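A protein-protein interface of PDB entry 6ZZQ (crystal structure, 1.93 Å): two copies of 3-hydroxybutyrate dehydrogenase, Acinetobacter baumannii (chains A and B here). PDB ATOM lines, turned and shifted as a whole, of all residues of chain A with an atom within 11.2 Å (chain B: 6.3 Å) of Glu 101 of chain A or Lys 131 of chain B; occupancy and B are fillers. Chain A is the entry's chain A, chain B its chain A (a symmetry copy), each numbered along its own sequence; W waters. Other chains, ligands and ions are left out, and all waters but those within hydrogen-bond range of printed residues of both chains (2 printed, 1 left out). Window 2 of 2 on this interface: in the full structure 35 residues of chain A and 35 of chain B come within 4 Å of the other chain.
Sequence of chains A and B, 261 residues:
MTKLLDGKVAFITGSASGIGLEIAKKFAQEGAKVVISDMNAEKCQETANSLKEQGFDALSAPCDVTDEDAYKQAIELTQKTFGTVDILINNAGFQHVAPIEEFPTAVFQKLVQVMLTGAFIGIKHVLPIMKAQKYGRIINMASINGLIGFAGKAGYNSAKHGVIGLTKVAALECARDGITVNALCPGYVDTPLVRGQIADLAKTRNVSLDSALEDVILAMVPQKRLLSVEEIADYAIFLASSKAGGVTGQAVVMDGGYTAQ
No position is printed for both chains. Of the 11 pairs that touch across the chains among the printed residues, none has its exchanged pair printed and touching as well.
Hydrophobic or aromatic side chains of chain B that line the printed part of chain A: Leu 127.
The side-chain hydroxyl of Thr 105 of chain A is in hydrogen-bond range of the side-chain amino group of Lys 124 of chain B, 3.2 Å away. O of Phe 103 of chain A sits close to NZ of Lys 124 of chain B (2.3 Å). The side-chain carboxylate of Glu 173 of chain B sits at hydrogen-bond distance from the backbone NH of Gly 152 of chain A (2.8 Å). The side-chain carboxylate (OE1) of Glu 173 of chain B is in hydrogen-bond range of the backbone NH (N) of Ile 100 of chain A (2.8 Å). NZ of Lys 131 of chain B lies within salt-bridge range of OE2 of Glu 101 of chain A (2.6 Å).
Water W2 lies within hydrogen-bond range of OE1 of Glu 173 of chain B (2.5 Å), OE1 of Glu 101 of chain A (2.6 Å) and NZ of Lys 131 of chain B (2.8 Å). Water W1 bridges the backbone NH of Thr 105 of chain A (3.0 Å) and the side-chain amino group of Lys 124 of chain B (3.4 Å).
Of chain B, only Lys 124 (3.9 Å), Leu 127 (3.9 Å) and Lys 131 (2.6 Å) come within 4 Å of Glu 101 of chain A. Lys 131 of chain B touches just one residue of chain A: Glu 101. Leu 127 of chain B touches one residue of chain A. No residue of chain A comes within 4 Å of Pro 128 of chain B. No residue of chain A comes within 4 Å of Ala 132 of chain B. No residue of chain A comes within 4 Å of Gln 133 of chain B. Glu 173 of chain B touches four residues of chain A. No residue of chain A comes within 4 Å of Cys 174 of chain B. No residue of chain A comes within 4 Å of Asp 177 of chain B. Of the printed residues of chain B, Phe 103 of chain A touches Lys 124 (2.3 Å). Of the printed residues of chain B, Thr 105 of chain A touches Lys 124 (3.2 Å). Of the printed residues of chain B, Ile 100 of chain A touches Lys 124 (3.3 Å) and Glu 173 (2.8 Å). Printed residues of chain B within 4 Å of Ala 151 of chain A: Glu 173. Val 107 of chain A touches none of the printed residues of chain B. Gly 155 of chain A touches none of the printed residues of chain B. The nearest residue of chain A that does not touch Lys 131 of chain B is Pro 99 of chain A (6.0 Å).
Among the printed residues, pairs that only touch across the chains: Pro 99 of chain A with Glu 173 of chain B (3.5 Å), Ile 100 of chain A with Lys 124 of chain B (3.3 Å), Glu 101 of chain A with Lys 124 of chain B (3.9 Å), Glu 101 of chain A with Leu 127 of chain B (3.9 Å), Pro 104 of chain A with Lys 124 of chain B (3.8 Å) and Ala 151 of chain A with Glu 173 of chain B (3.9 Å).
The backbone NH of Ala 98 of chain A is in hydrogen-bond range of the backbone carbonyl oxygen of Gly 152 of chain A, 2.9 Å away.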
ATOM      1  N   HIS A  96      26.538  31.905  26.078  1.00  0.00           N
ATOM      2  CA  HIS A  96      27.092  31.626  24.732  1.00  0.00           C
ATOM      3  C   HIS A  96      26.027  30.911  23.900  1.00  0.00           C
ATOM      4  O   HIS A  96      25.749  29.760  24.229  1.00  0.00           O
ATOM      5  CB  HIS A  96      28.366  30.787  24.814  1.00  0.00           C
ATOM      6  CG  HIS A  96      29.110  30.728  23.519  1.00  0.00           C
ATOM      7  ND1 HIS A  96      30.192  31.539  23.251  1.00  0.00           N
ATOM      8  CD2 HIS A  96      28.924  29.973  22.413  1.00  0.00           C
ATOM      9  CE1 HIS A  96      30.647  31.282  22.044  1.00  0.00           C
ATOM     10  NE2 HIS A  96      29.886  30.318  21.511  1.00  0.00           N
ATOM     11  N   VAL A  97      25.451  31.596  22.901  1.00  0.00           N
ATOM     12  CA  VAL A  97      24.432  31.074  21.927  1.00  0.00           C
ATOM     13  C   VAL A  97      25.156  30.561  20.667  1.00  0.00           C
ATOM     14  O   VAL A  97      25.800  31.409  19.997  1.00  0.00           O
ATOM     15  CB  VAL A  97      23.430  32.184  21.555  1.00  0.00           C
ATOM     16  CG1 VAL A  97      22.343  31.702  20.598  1.00  0.00           C
ATOM     17  CG2 VAL A  97      22.813  32.844  22.780  1.00  0.00           C
ATOM     18  N   ALA A  98      25.049  29.255  20.356  1.00  0.00           N
ATOM     19  CA  ALA A  98      25.531  28.591  19.114  1.00  0.00           C
ATOM     20  C   ALA A  98      24.728  27.327  18.836  1.00  0.00           C
ATOM     21  O   ALA A  98      24.291  26.670  19.771  1.00  0.00           O
ATOM     22  CB  ALA A  98      26.983  28.221  19.238  1.00  0.00           C
ATOM     23  N   PRO A  99      24.555  26.910  17.556  1.00  0.00           N
ATOM     24  CA  PRO A  99      24.034  25.583  17.238  1.00  0.00           C
ATOM     25  C   PRO A  99      24.986  24.568  17.856  1.00  0.00           C
ATOM     26  O   PRO A  99      26.176  24.875  17.909  1.00  0.00           O
ATOM     27  CB  PRO A  99      24.108  25.452  15.707  1.00  0.00           C
ATOM     28  CG  PRO A  99      24.235  26.891  15.218  1.00  0.00           C
ATOM     29  CD  PRO A  99      24.908  27.660  16.343  1.00  0.00           C
ATOM     30  N   ILE A 100      24.457  23.413  18.274  1.00  0.00           N
ATOM     31  CA  ILE A 100      25.221  22.378  19.023  1.00  0.00           C
ATOM     32  C   ILE A 100      26.463  22.002  18.212  1.00  0.00           C
ATOM     33  O   ILE A 100      27.540  21.850  18.810  1.00  0.00           O
ATOM     34  CB  ILE A 100      24.324  21.167  19.332  1.00  0.00           C
ATOM     35  CG1 ILE A 100      23.412  21.458  20.528  1.00  0.00           C
ATOM     36  CG2 ILE A 100      25.150  19.914  19.550  1.00  0.00           C
ATOM     37  CD1 ILE A 100      22.281  20.476  20.694  1.00  0.00           C
ATOM     38  N   GLU A 101      26.328  21.854  16.890  1.00  0.00           N
ATOM     39  CA  GLU A 101      27.450  21.374  16.036  1.00  0.00           C
ATOM     40  C   GLU A 101      28.639  22.334  16.157  1.00  0.00           C
ATOM     41  O   GLU A 101      29.753  21.833  16.091  1.00  0.00           O
ATOM     42  CB  GLU A 101      27.044  21.220  14.572  1.00  0.00           C
ATOM     43  CG  GLU A 101      25.938  20.214  14.369  1.00  0.00           C
ATOM     44  CD  GLU A 101      24.550  20.822  14.374  1.00  0.00           C
ATOM     45  OE1 GLU A 101      24.333  21.864  15.063  1.00  0.00           O
ATOM     46  OE2 GLU A 101      23.685  20.265  13.675  1.00  0.00           O
ATOM     47  N   GLU A 102      28.392  23.633  16.328  1.00  0.00           N
ATOM     48  CA  GLU A 102      29.433  24.696  16.420  1.00  0.00           C
ATOM     49  C   GLU A 102      29.573  25.156  17.884  1.00  0.00           C
ATOM     50  O   GLU A 102      29.959  26.314  18.097  1.00  0.00           O
ATOM     51  CB  GLU A 102      29.071  25.915  15.569  1.00  0.00           C
ATOM     52  CG  GLU A 102      28.575  25.627  14.150  1.00  0.00           C
ATOM     53  CD  GLU A 102      27.683  26.723  13.554  1.00  0.00           C
ATOM     54  OE1 GLU A 102      27.723  27.881  14.057  1.00  0.00           O
ATOM     55  OE2 GLU A 102      26.921  26.424  12.601  1.00  0.00           O
ATOM     56  N   PHE A 103      29.201  24.324  18.861  1.00  0.00           N
ATOM     57  CA  PHE A 103      29.191  24.726  20.296  1.00  0.00           C
ATOM     58  C   PHE A 103      30.460  24.138  20.905  1.00  0.00           C
ATOM     59  O   PHE A 103      30.548  22.920  21.053  1.00  0.00           O
ATOM     60  CB  PHE A 103      27.881  24.298  20.989  1.00  0.00           C
ATOM     61  CG  PHE A 103      27.533  25.098  22.227  1.00  0.00           C
ATOM     62  CD1 PHE A 103      28.365  25.099  23.337  1.00  0.00           C
ATOM     63  CD2 PHE A 103      26.408  25.901  22.258  1.00  0.00           C
ATOM     64  CE1 PHE A 103      28.074  25.889  24.443  1.00  0.00           C
ATOM     65  CE2 PHE A 103      26.112  26.685  23.366  1.00  0.00           C
ATOM     66  CZ  PHE A 103      26.941  26.666  24.464  1.00  0.00           C
ATOM     67  N   PRO A 104      31.531  24.925  21.161  1.00  0.00           N
ATOM     68  CA  PRO A 104      32.774  24.348  21.675  1.00  0.00           C
ATOM     69  C   PRO A 104      32.473  23.636  23.004  1.00  0.00           C
ATOM     70  O   PRO A 104      31.811  24.220  23.842  1.00  0.00           O
ATOM     71  CB  PRO A 104      33.719  25.543  21.881  1.00  0.00           C
ATOM     72  CG  PRO A 104      33.106  26.643  21.051  1.00  0.00           C
ATOM     73  CD  PRO A 104      31.603  26.395  21.086  1.00  0.00           C
ATOM     74  N   THR A 105      32.943  22.404  23.140  1.00  0.00           N
ATOM     75  CA  THR A 105      32.753  21.551  24.333  1.00  0.00           C
ATOM     76  C   THR A 105      33.312  22.256  25.570  1.00  0.00           C
ATOM     77  O   THR A 105      32.676  22.142  26.630  1.00  0.00           O
ATOM     78  CB  THR A 105      33.412  20.194  24.103  1.00  0.00           C
ATOM     79  OG1 THR A 105      32.854  19.655  22.906  1.00  0.00           O
ATOM     80  CG2 THR A 105      33.198  19.236  25.251  1.00  0.00           C
ATOM     81  N   ALA A 106      34.455  22.947  25.442  1.00  0.00           N
ATOM     82  CA  ALA A 106      35.094  23.707  26.541  1.00  0.00           C
ATOM     83  C   ALA A 106      34.092  24.725  27.103  1.00  0.00           C
ATOM     84  O   ALA A 106      34.042  24.920  28.345  1.00  0.00           O
ATOM     85  CB  ALA A 106      36.353  24.399  26.042  1.00  0.00           C
ATOM     86  N   VAL A 107      33.367  25.399  26.211  1.00  0.00           N
ATOM     87  CA  VAL A 107      32.433  26.507  26.539  1.00  0.00           C
ATOM     88  C   VAL A 107      31.176  25.903  27.171  1.00  0.00           C
ATOM     89  O   VAL A 107      30.739  26.414  28.214  1.00  0.00           O
ATOM     90  CB  VAL A 107      32.141  27.350  25.286  1.00  0.00           C
ATOM     91  CG1 VAL A 107      31.044  28.376  25.514  1.00  0.00           C
ATOM     92  CG2 VAL A 107      33.423  28.013  24.781  1.00  0.00           C
ATOM     93  N   PHE A 108      30.647  24.824  26.603  1.00  0.00           N
ATOM     94  CA  PHE A 108      29.598  24.017  27.266  1.00  0.00           C
ATOM     95  C   PHE A 108      29.993  23.748  28.734  1.00  0.00           C
ATOM     96  O   PHE A 108      29.218  24.077  29.656  1.00  0.00           O
ATOM     97  CB  PHE A 108      29.418  22.673  26.585  1.00  0.00           C
ATOM     98  CG  PHE A 108      28.255  21.891  27.124  1.00  0.00           C
ATOM     99  CD1 PHE A 108      26.978  22.092  26.615  1.00  0.00           C
ATOM    100  CD2 PHE A 108      28.442  20.922  28.096  1.00  0.00           C
ATOM    101  CE1 PHE A 108      25.913  21.341  27.083  1.00  0.00           C
ATOM    102  CE2 PHE A 108      27.371  20.182  28.572  1.00  0.00           C
ATOM    103  CZ  PHE A 108      26.110  20.386  28.062  1.00  0.00           C
ATOM    104  N   ALA A 151      16.590  26.842  21.180  1.00  0.00           N
ATOM    105  CA  ALA A 151      17.625  26.476  20.182  1.00  0.00           C
ATOM    106  C   ALA A 151      18.852  27.385  20.355  1.00  0.00           C
ATOM    107  O   ALA A 151      18.689  28.622  20.539  1.00  0.00           O
ATOM    108  CB  ALA A 151      17.062  26.574  18.784  1.00  0.00           C
ATOM    109  N   GLY A 152      20.043  26.804  20.312  1.00  0.00           N
ATOM    110  CA  GLY A 152      21.304  27.561  20.442  1.00  0.00           C
ATOM    111  C   GLY A 152      21.806  27.671  21.882  1.00  0.00           C
ATOM    112  O   GLY A 152      22.929  28.180  22.043  1.00  0.00           O
ATOM    113  N   LYS A 153      21.071  27.179  22.893  1.00  0.00           N
ATOM    114  CA  LYS A 153      21.461  27.409  24.320  1.00  0.00           C
ATOM    115  C   LYS A 153      21.748  26.082  25.022  1.00  0.00           C
ATOM    116  O   LYS A 153      21.251  25.895  26.170  1.00  0.00           O
ATOM    117  CB  LYS A 153      20.364  28.216  25.024  1.00  0.00           C
ATOM    118  CG  LYS A 153      20.293  29.667  24.589  1.00  0.00           C
ATOM    119  CD  LYS A 153      19.155  30.445  25.166  1.00  0.00           C
ATOM    120  CE  LYS A 153      19.277  31.916  24.862  1.00  0.00           C
ATOM    121  NZ  LYS A 153      17.977  32.604  24.953  1.00  0.00           N
ATOM    122  N   ALA A 154      22.508  25.202  24.364  1.00  0.00           N
ATOM    123  CA  ALA A 154      22.822  23.835  24.837  1.00  0.00           C
ATOM    124  C   ALA A 154      23.388  23.913  26.267  1.00  0.00           C
ATOM    125  O   ALA A 154      22.818  23.271  27.201  1.00  0.00           O
ATOM    126  CB  ALA A 154      23.787  23.190  23.890  1.00  0.00           C
ATOM    127  N   GLY A 155      24.450  24.703  26.434  1.00  0.00           N
ATOM    128  CA  GLY A 155      25.173  24.846  27.715  1.00  0.00           C
ATOM    129  C   GLY A 155      24.343  25.576  28.751  1.00  0.00           C
ATOM    130  O   GLY A 155      24.271  25.107  29.911  1.00  0.00           O
ATOM    131  N   ILE B 123      25.910  13.770  20.951  1.00  0.00           N
ATOM    132  CA  ILE B 123      24.880  14.444  20.122  1.00  0.00           C
ATOM    133  C   ILE B 123      25.629  15.322  19.111  1.00  0.00           C
ATOM    134  O   ILE B 123      25.344  15.207  17.886  1.00  0.00           O
ATOM    135  CB  ILE B 123      23.873  15.237  20.981  1.00  0.00           C
ATOM    136  CG1 ILE B 123      23.036  14.311  21.873  1.00  0.00           C
ATOM    137  CG2 ILE B 123      22.989  16.116  20.104  1.00  0.00           C
ATOM    138  CD1 ILE B 123      22.138  15.028  22.870  1.00  0.00           C
ATOM    139  N   LYS B 124      26.550  16.164  19.585  1.00  0.00           N
ATOM    140  CA  LYS B 124      27.366  17.032  18.706  1.00  0.00           C
ATOM    141  C   LYS B 124      27.917  16.235  17.515  1.00  0.00           C
ATOM    142  O   LYS B 124      27.879  16.780  16.374  1.00  0.00           O
ATOM    143  CB  LYS B 124      28.550  17.648  19.452  1.00  0.00           C
ATOM    144  CG  LYS B 124      29.421  18.521  18.571  1.00  0.00           C
ATOM    145  CD  LYS B 124      30.612  19.074  19.309  1.00  0.00           C
ATOM    146  CE  LYS B 124      30.431  20.513  19.706  1.00  0.00           C
ATOM    147  NZ  LYS B 124      31.696  21.025  20.276  1.00  0.00           N
ATOM    148  N   VAL B 126      26.903  13.035  16.325  1.00  0.00           N
ATOM    149  CA  VAL B 126      25.943  12.267  15.469  1.00  0.00           C
ATOM    150  C   VAL B 126      25.017  13.228  14.717  1.00  0.00           C
ATOM    151  O   VAL B 126      24.448  12.792  13.710  1.00  0.00           O
ATOM    152  CB  VAL B 126      25.123  11.214  16.231  1.00  0.00           C
ATOM    153  CG1 VAL B 126      26.019  10.163  16.859  1.00  0.00           C
ATOM    154  CG2 VAL B 126      24.182  11.860  17.235  1.00  0.00           C
ATOM    155  N   LEU B 127      24.878  14.485  15.136  1.00  0.00           N
ATOM    156  CA  LEU B 127      23.850  15.373  14.525  1.00  0.00           C
ATOM    157  C   LEU B 127      24.163  15.589  13.040  1.00  0.00           C
ATOM    158  O   LEU B 127      23.250  15.512  12.208  1.00  0.00           O
ATOM    159  CB  LEU B 127      23.738  16.683  15.308  1.00  0.00           C
ATOM    160  CG  LEU B 127      22.627  16.730  16.365  1.00  0.00           C
ATOM    161  CD1 LEU B 127      22.568  18.115  16.999  1.00  0.00           C
ATOM    162  CD2 LEU B 127      21.266  16.383  15.774  1.00  0.00           C
ATOM    163  N   PRO B 128      25.447  15.800  12.645  1.00  0.00           N
ATOM    164  CA  PRO B 128      25.817  15.906  11.229  1.00  0.00           C
ATOM    165  C   PRO B 128      25.364  14.713  10.376  1.00  0.00           C
ATOM    166  O   PRO B 128      24.869  14.937   9.308  1.00  0.00           O
ATOM    167  CB  PRO B 128      27.359  15.952  11.248  1.00  0.00           C
ATOM    168  CG  PRO B 128      27.703  16.521  12.624  1.00  0.00           C
ATOM    169  CD  PRO B 128      26.615  15.971  13.530  1.00  0.00           C
ATOM    170  N   ILE B 129      25.625  13.493  10.842  1.00  0.00           N
ATOM    171  CA  ILE B 129      25.319  12.217  10.141  1.00  0.00           C
ATOM    172  C   ILE B 129      23.799  12.110   9.952  1.00  0.00           C
ATOM    173  O   ILE B 129      23.329  11.690   8.870  1.00  0.00           O
ATOM    174  CB  ILE B 129      25.914  11.045  10.946  1.00  0.00           C
ATOM    175  CG1 ILE B 129      27.443  11.111  11.002  1.00  0.00           C
ATOM    176  CG2 ILE B 129      25.468   9.706  10.396  1.00  0.00           C
ATOM    177  CD1 ILE B 129      28.065  10.254  12.091  1.00  0.00           C
ATOM    178  N   MET B 130      23.046  12.456  10.991  1.00  0.00           N
ATOM    179  CA  MET B 130      21.570  12.334  11.021  1.00  0.00           C
ATOM    180  C   MET B 130      20.948  13.446  10.175  1.00  0.00           C
ATOM    181  O   MET B 130      20.020  13.155   9.407  1.00  0.00           O
ATOM    182  CB  MET B 130      21.065  12.407  12.468  1.00  0.00           C
ATOM    183  CG  MET B 130      21.556  11.237  13.328  1.00  0.00           C
ATOM    184  SD  MET B 130      20.921  11.270  15.038  1.00  0.00           S
ATOM    185  CE  MET B 130      21.216   9.575  15.532  1.00  0.00           C
ATOM    186  N   LYS B 131      21.445  14.677  10.281  1.00  0.00           N
ATOM    187  CA  LYS B 131      20.892  15.814   9.512  1.00  0.00           C
ATOM    188  C   LYS B 131      21.108  15.593   8.001  1.00  0.00           C
ATOM    189  O   LYS B 131      20.177  15.858   7.234  1.00  0.00           O
ATOM    190  CB  LYS B 131      21.474  17.130  10.023  1.00  0.00           C
ATOM    191  CG  LYS B 131      20.873  17.587  11.340  1.00  0.00           C
ATOM    192  CD  LYS B 131      21.463  18.859  11.875  1.00  0.00           C
ATOM    193  CE  LYS B 131      20.543  19.572  12.845  1.00  0.00           C
ATOM    194  NZ  LYS B 131      21.162  20.800  13.393  1.00  0.00           N
ATOM    195  N   ALA B 132      22.273  15.090   7.600  1.00  0.00           N
ATOM    196  CA  ALA B 132      22.584  14.737   6.195  1.00  0.00           C
ATOM    197  C   ALA B 132      21.501  13.777   5.656  1.00  0.00           C
ATOM    198  O   ALA B 132      20.982  14.057   4.552  1.00  0.00           O
ATOM    199  CB  ALA B 132      23.975  14.167   6.096  1.00  0.00           C
ATOM    200  N   GLN B 133      21.122  12.738   6.422  1.00  0.00           N
ATOM    201  CA  GLN B 133      20.204  11.654   5.965  1.00  0.00           C
ATOM    202  C   GLN B 133      18.752  12.023   6.274  1.00  0.00           C
ATOM    203  O   GLN B 133      17.850  11.253   5.900  1.00  0.00           O
ATOM    204  CB  GLN B 133      20.634  10.305   6.534  1.00  0.00           C
ATOM    205  CG  GLN B 133      20.362  10.092   8.017  1.00  0.00           C
ATOM    206  CD  GLN B 133      20.884   8.750   8.452  1.00  0.00           C
ATOM    207  OE1 GLN B 133      21.617   8.100   7.710  1.00  0.00           O
ATOM    208  NE2 GLN B 133      20.526   8.328   9.660  1.00  0.00           N
ATOM    209  N   LYS B 134      18.528  13.190   6.882  1.00  0.00           N
ATOM    210  CA  LYS B 134      17.207  13.647   7.377  1.00  0.00           C
ATOM    211  C   LYS B 134      16.513  12.528   8.161  1.00  0.00           C
ATOM    212  O   LYS B 134      15.276  12.428   8.040  1.00  0.00           O
ATOM    213  CB  LYS B 134      16.287  14.089   6.235  1.00  0.00           C
ATOM    214  CG  LYS B 134      16.806  15.239   5.398  1.00  0.00           C
ATOM    215  CD  LYS B 134      16.819  16.529   6.144  1.00  0.00           C
ATOM    216  CE  LYS B 134      17.162  17.698   5.250  1.00  0.00           C
ATOM    217  NZ  LYS B 134      17.137  18.971   6.003  1.00  0.00           N
ATOM    218  N   TYR B 135      17.252  11.739   8.953  1.00  0.00           N
ATOM    219  CA  TYR B 135      16.646  10.765   9.898  1.00  0.00           C
ATOM    220  C   TYR B 135      17.541  10.572  11.124  1.00  0.00           C
ATOM    221  O   TYR B 135      18.757  10.342  10.990  1.00  0.00           O
ATOM    222  CB  TYR B 135      16.441   9.382   9.271  1.00  0.00           C
ATOM    223  CG  TYR B 135      15.640   8.435  10.134  1.00  0.00           C
ATOM    224  CD1 TYR B 135      14.258   8.550  10.223  1.00  0.00           C
ATOM    225  CD2 TYR B 135      16.255   7.453  10.885  1.00  0.00           C
ATOM    226  CE1 TYR B 135      13.506   7.705  11.018  1.00  0.00           C
ATOM    227  CE2 TYR B 135      15.516   6.608  11.702  1.00  0.00           C
ATOM    228  CZ  TYR B 135      14.139   6.739  11.776  1.00  0.00           C
ATOM    229  OH  TYR B 135      13.396   5.900  12.565  1.00  0.00           O
ATOM    230  N   GLU B 173      16.576  22.102  17.853  1.00  0.00           N
ATOM    231  CA  GLU B 173      17.585  22.364  16.800  1.00  0.00           C
ATOM    232  C   GLU B 173      17.403  21.416  15.600  1.00  0.00           C
ATOM    233  O   GLU B 173      17.963  21.731  14.541  1.00  0.00           O
ATOM    234  CB  GLU B 173      18.999  22.293  17.374  1.00  0.00           C
ATOM    235  CG  GLU B 173      19.356  23.528  18.205  1.00  0.00           C
ATOM    236  CD  GLU B 173      20.794  23.600  18.727  1.00  0.00           C
ATOM    237  OE1 GLU B 173      21.701  23.046  18.085  1.00  0.00           O
ATOM    238  OE2 GLU B 173      20.994  24.193  19.812  1.00  0.00           O
ATOM    239  N   CYS B 174      16.733  20.273  15.745  1.00  0.00           N
ATOM    240  CA  CYS B 174      16.650  19.266  14.649  1.00  0.00           C
ATOM    241  C   CYS B 174      15.195  18.832  14.350  1.00  0.00           C
ATOM    242  O   CYS B 174      14.983  17.861  13.604  1.00  0.00           O
ATOM    243  CB  CYS B 174      17.562  18.106  15.002  1.00  0.00           C
ATOM    244  SG  CYS B 174      16.991  17.165  16.439  1.00  0.00           S
ATOM    245  N   ASP B 177      14.429  18.101  10.719  1.00  0.00           N
ATOM    246  CA  ASP B 177      15.487  17.314  10.045  1.00  0.00           C
ATOM    247  C   ASP B 177      15.190  15.817  10.138  1.00  0.00           C
ATOM    248  O   ASP B 177      16.114  15.046   9.838  1.00  0.00           O
ATOM    249  CB  ASP B 177      16.863  17.676  10.619  1.00  0.00           C
ATOM    250  CG  ASP B 177      17.259  19.122  10.349  1.00  0.00           C
ATOM    251  OD1 ASP B 177      17.299  19.495   9.172  1.00  0.00           O
ATOM    252  OD2 ASP B 177      17.471  19.875  11.317  1.00  0.00           O
ATOM    253  N   ILE B 179      14.572  14.125  12.865  1.00  0.00           N
ATOM    254  CA  ILE B 179      15.356  13.673  14.042  1.00  0.00           C
ATOM    255  C   ILE B 179      14.578  13.986  15.315  1.00  0.00           C
ATOM    256  O   ILE B 179      14.158  15.148  15.483  1.00  0.00           O
ATOM    257  CB  ILE B 179      16.741  14.338  14.075  1.00  0.00           C
ATOM    258  CG1 ILE B 179      17.534  14.024  12.804  1.00  0.00           C
ATOM    259  CG2 ILE B 179      17.486  13.871  15.325  1.00  0.00           C
ATOM    260  CD1 ILE B 179      18.788  14.835  12.638  1.00  0.00           C
HETATM  261  O   HOH W   1      34.892  21.788  20.948  1.00  0.00           O
HETATM  262  O   HOH W   2      21.809  22.151  15.738  1.00  0.00           O
